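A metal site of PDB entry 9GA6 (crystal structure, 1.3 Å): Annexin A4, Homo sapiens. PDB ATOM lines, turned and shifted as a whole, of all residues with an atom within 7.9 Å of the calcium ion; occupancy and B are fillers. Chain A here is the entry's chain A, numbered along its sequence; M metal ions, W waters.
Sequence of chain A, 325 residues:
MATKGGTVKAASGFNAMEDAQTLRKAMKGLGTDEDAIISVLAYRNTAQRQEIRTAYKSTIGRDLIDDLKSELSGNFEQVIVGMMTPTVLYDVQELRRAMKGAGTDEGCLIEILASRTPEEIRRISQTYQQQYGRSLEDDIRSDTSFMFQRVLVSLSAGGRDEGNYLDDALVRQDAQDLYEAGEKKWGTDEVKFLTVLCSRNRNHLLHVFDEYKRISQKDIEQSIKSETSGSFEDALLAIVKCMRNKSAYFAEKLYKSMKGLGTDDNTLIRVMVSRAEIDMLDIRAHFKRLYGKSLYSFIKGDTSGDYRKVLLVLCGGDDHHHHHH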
ATOM      1  N   ARG A  24     -16.020   5.847  36.254  1.00  0.00           N
ATOM      2  CA  ARG A  24     -16.611   7.129  35.889  1.00  0.00           C
ATOM      3  C   ARG A  24     -15.691   7.899  34.952  1.00  0.00           C
ATOM      4  O   ARG A  24     -16.182   8.430  33.959  1.00  0.00           O
ATOM      5  CB  ARG A  24     -17.044   7.920  37.134  1.00  0.00           C
ATOM      6  CG  ARG A  24     -17.486   9.355  36.882  1.00  0.00           C
ATOM      7  CD  ARG A  24     -18.701   9.413  36.019  1.00  0.00           C
ATOM      8  NE  ARG A  24     -19.213  10.783  35.984  1.00  0.00           N
ATOM      9  CZ  ARG A  24     -19.889  11.321  34.990  1.00  0.00           C
ATOM     10  NH1 ARG A  24     -20.306  10.623  33.964  1.00  0.00           N
ATOM     11  NH2 ARG A  24     -20.203  12.612  35.124  1.00  0.00           N
ATOM     12  N   LYS A  25     -14.417   8.013  35.296  1.00  0.00           N
ATOM     13  CA  LYS A  25     -13.488   8.747  34.452  1.00  0.00           C
ATOM     14  C   LYS A  25     -13.409   8.137  33.065  1.00  0.00           C
ATOM     15  O   LYS A  25     -13.354   8.877  32.076  1.00  0.00           O
ATOM     16  CB  LYS A  25     -12.074   8.739  35.042  1.00  0.00           C
ATOM     17  CG  LYS A  25     -11.921   9.597  36.322  1.00  0.00           C
ATOM     18  CD  LYS A  25     -11.715  11.069  36.022  1.00  0.00           C
ATOM     19  CE  LYS A  25     -11.336  11.769  37.296  1.00  0.00           C
ATOM     20  NZ  LYS A  25     -11.046  13.172  37.003  1.00  0.00           N
ATOM     21  N   ALA A  26     -13.542   6.810  32.943  1.00  0.00           N
ATOM     22  CA  ALA A  26     -13.485   6.144  31.649  1.00  0.00           C
ATOM     23  C   ALA A  26     -14.678   6.538  30.768  1.00  0.00           C
ATOM     24  O   ALA A  26     -14.550   6.511  29.531  1.00  0.00           O
ATOM     25  CB  ALA A  26     -13.451   4.639  31.839  1.00  0.00           C
ATOM     26  N   MET A  27     -15.847   6.844  31.342  1.00  0.00           N
ATOM     27  CA  MET A  27     -17.075   7.096  30.623  1.00  0.00           C
ATOM     28  C   MET A  27     -17.411   8.597  30.506  1.00  0.00           C
ATOM     29  O   MET A  27     -18.054   8.969  29.523  1.00  0.00           O
ATOM     30  CB  MET A  27     -18.238   6.330  31.238  1.00  0.00           C
ATOM     31  CG  MET A  27     -18.092   4.848  31.099  1.00  0.00           C
ATOM     32  SD  MET A  27     -19.441   3.853  31.756  1.00  0.00           S
ATOM     33  CE  MET A  27     -18.989   3.933  33.486  1.00  0.00           C
ATOM     34  N   LYS A  28     -17.010   9.411  31.480  1.00  0.00           N
ATOM     35  CA  LYS A  28     -17.391  10.830  31.460  1.00  0.00           C
ATOM     36  C   LYS A  28     -16.878  11.505  30.196  1.00  0.00           C
ATOM     37  O   LYS A  28     -15.725  11.392  29.852  1.00  0.00           O
ATOM     38  CB  LYS A  28     -16.854  11.509  32.714  1.00  0.00           C
ATOM     39  CG  LYS A  28     -17.280  12.949  32.826  1.00  0.00           C
ATOM     40  CD  LYS A  28     -16.921  13.597  34.131  1.00  0.00           C
ATOM     41  CE  LYS A  28     -17.494  14.983  34.203  1.00  0.00           C
ATOM     42  NZ  LYS A  28     -16.961  15.670  35.366  1.00  0.00           N
ATOM     43  N   GLY A  29     -17.747  12.305  29.580  1.00  0.00           N
ATOM     44  CA  GLY A  29     -17.336  13.090  28.424  1.00  0.00           C
ATOM     45  C   GLY A  29     -17.525  12.325  27.137  1.00  0.00           C
ATOM     46  O   GLY A  29     -17.860  11.145  27.099  1.00  0.00           O
ATOM     47  N   LEU A  30     -17.298  13.002  25.995  1.00  0.00           N
ATOM     48  CA  LEU A  30     -17.418  12.332  24.718  1.00  0.00           C
ATOM     49  C   LEU A  30     -16.503  11.115  24.668  1.00  0.00           C
ATOM     50  O   LEU A  30     -15.357  11.145  25.097  1.00  0.00           O
ATOM     51  CB  LEU A  30     -17.055  13.327  23.605  1.00  0.00           C
ATOM     52  CG  LEU A  30     -17.212  12.811  22.162  1.00  0.00           C
ATOM     53  CD1 LEU A  30     -18.558  12.234  21.800  1.00  0.00           C
ATOM     54  CD2 LEU A  30     -16.848  13.923  21.185  1.00  0.00           C
ATOM     55  N   GLY A  31     -17.085  10.036  24.176  1.00  0.00           N
ATOM     56  CA  GLY A  31     -16.382   8.783  23.988  1.00  0.00           C
ATOM     57  C   GLY A  31     -16.206   7.985  25.273  1.00  0.00           C
ATOM     58  O   GLY A  31     -16.808   8.330  26.279  1.00  0.00           O
ATOM     59  N   THR A  32     -15.391   6.949  25.200  1.00  0.00           N
ATOM     60  CA  THR A  32     -15.218   5.992  26.281  1.00  0.00           C
ATOM     61  C   THR A  32     -13.801   5.474  26.242  1.00  0.00           C
ATOM     62  O   THR A  32     -13.202   5.247  25.168  1.00  0.00           O
ATOM     63  CB  THR A  32     -16.169   4.805  26.004  1.00  0.00           C
ATOM     64  OG1 THR A  32     -17.457   5.290  25.711  1.00  0.00           O
ATOM     65  CG2 THR A  32     -16.250   3.840  27.169  1.00  0.00           C
ATOM     66  N   ASP A  33     -13.235   5.164  27.410  1.00  0.00           N
ATOM     67  CA  ASP A  33     -12.006   4.410  27.536  1.00  0.00           C
ATOM     68  C   ASP A  33     -12.366   2.944  27.833  1.00  0.00           C
ATOM     69  O   ASP A  33     -12.382   2.540  28.993  1.00  0.00           O
ATOM     70  CB  ASP A  33     -11.076   4.981  28.600  1.00  0.00           C
ATOM     71  CG  ASP A  33      -9.741   4.297  28.697  1.00  0.00           C
ATOM     72  OD1 ASP A  33      -9.530   3.283  28.020  1.00  0.00           O
ATOM     73  OD2 ASP A  33      -8.899   4.846  29.481  1.00  0.00           O
ATOM     74  N   ASP A  67     -24.966   3.377  33.043  1.00  0.00           N
ATOM     75  CA  ASP A  67     -23.907   4.089  32.345  1.00  0.00           C
ATOM     76  C   ASP A  67     -23.213   3.163  31.348  1.00  0.00           C
ATOM     77  O   ASP A  67     -22.943   3.561  30.215  1.00  0.00           O
ATOM     78  CB  ASP A  67     -22.898   4.692  33.333  1.00  0.00           C
ATOM     79  CG  ASP A  67     -23.334   5.972  34.014  1.00  0.00           C
ATOM     80  OD1 ASP A  67     -24.451   6.500  33.628  1.00  0.00           O
ATOM     81  OD2 ASP A  67     -22.565   6.503  34.841  1.00  0.00           O
ATOM     82  N   SER A  70     -25.332   2.705  28.301  1.00  0.00           N
ATOM     83  CA  SER A  70     -25.348   3.927  27.498  1.00  0.00           C
ATOM     84  C   SER A  70     -24.071   4.061  26.691  1.00  0.00           C
ATOM     85  O   SER A  70     -24.095   4.545  25.557  1.00  0.00           O
ATOM     86  CB  SER A  70     -25.543   5.151  28.357  1.00  0.00           C
ATOM     87  OG  SER A  70     -25.539   6.351  27.581  1.00  0.00           O
ATOM     88  N   GLU A  71     -22.937   3.715  27.268  1.00  0.00           N
ATOM     89  CA  GLU A  71     -21.645   3.980  26.659  1.00  0.00           C
ATOM     90  C   GLU A  71     -21.195   2.885  25.689  1.00  0.00           C
ATOM     91  O   GLU A  71     -20.468   3.176  24.742  1.00  0.00           O
ATOM     92  CB  GLU A  71     -20.597   4.100  27.762  1.00  0.00           C
ATOM     93  CG  GLU A  71     -20.814   5.353  28.581  1.00  0.00           C
ATOM     94  CD  GLU A  71     -20.098   6.597  28.120  1.00  0.00           C
ATOM     95  OE1 GLU A  71     -18.971   6.524  27.584  1.00  0.00           O
ATOM     96  OE2 GLU A  71     -20.645   7.675  28.362  1.00  0.00           O
HETATM   97 CA    CA M   1     -18.850   9.031  27.357  1.00  0.00          CA
HETATM   98  O   HOH W   1     -19.909   8.687  25.283  1.00  0.00           O
HETATM   99  O   HOH W   2     -20.654  10.569  27.804  1.00  0.00           O
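The side-chain carboxylate of Glu 71 lies close to the side-chain hydroxyl of Thr 32, 2.7 Å away.
Within 4 Å of the calcium ion: Met 27, Gly 29, Gly 31 and Glu 71.
The calcium ion is bound by the backbone carbonyl oxygen (O) of Met 27, the backbone carbonyl oxygen (O) of Gly 29, water W1, water W2, the backbone carbonyl oxygen (O) of Gly 31, the side-chain carboxylate (OE2) of Glu 71 and the side-chain carboxylate (OE1) of Glu 71. The calcium ion has seven donor atoms within binding distance.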
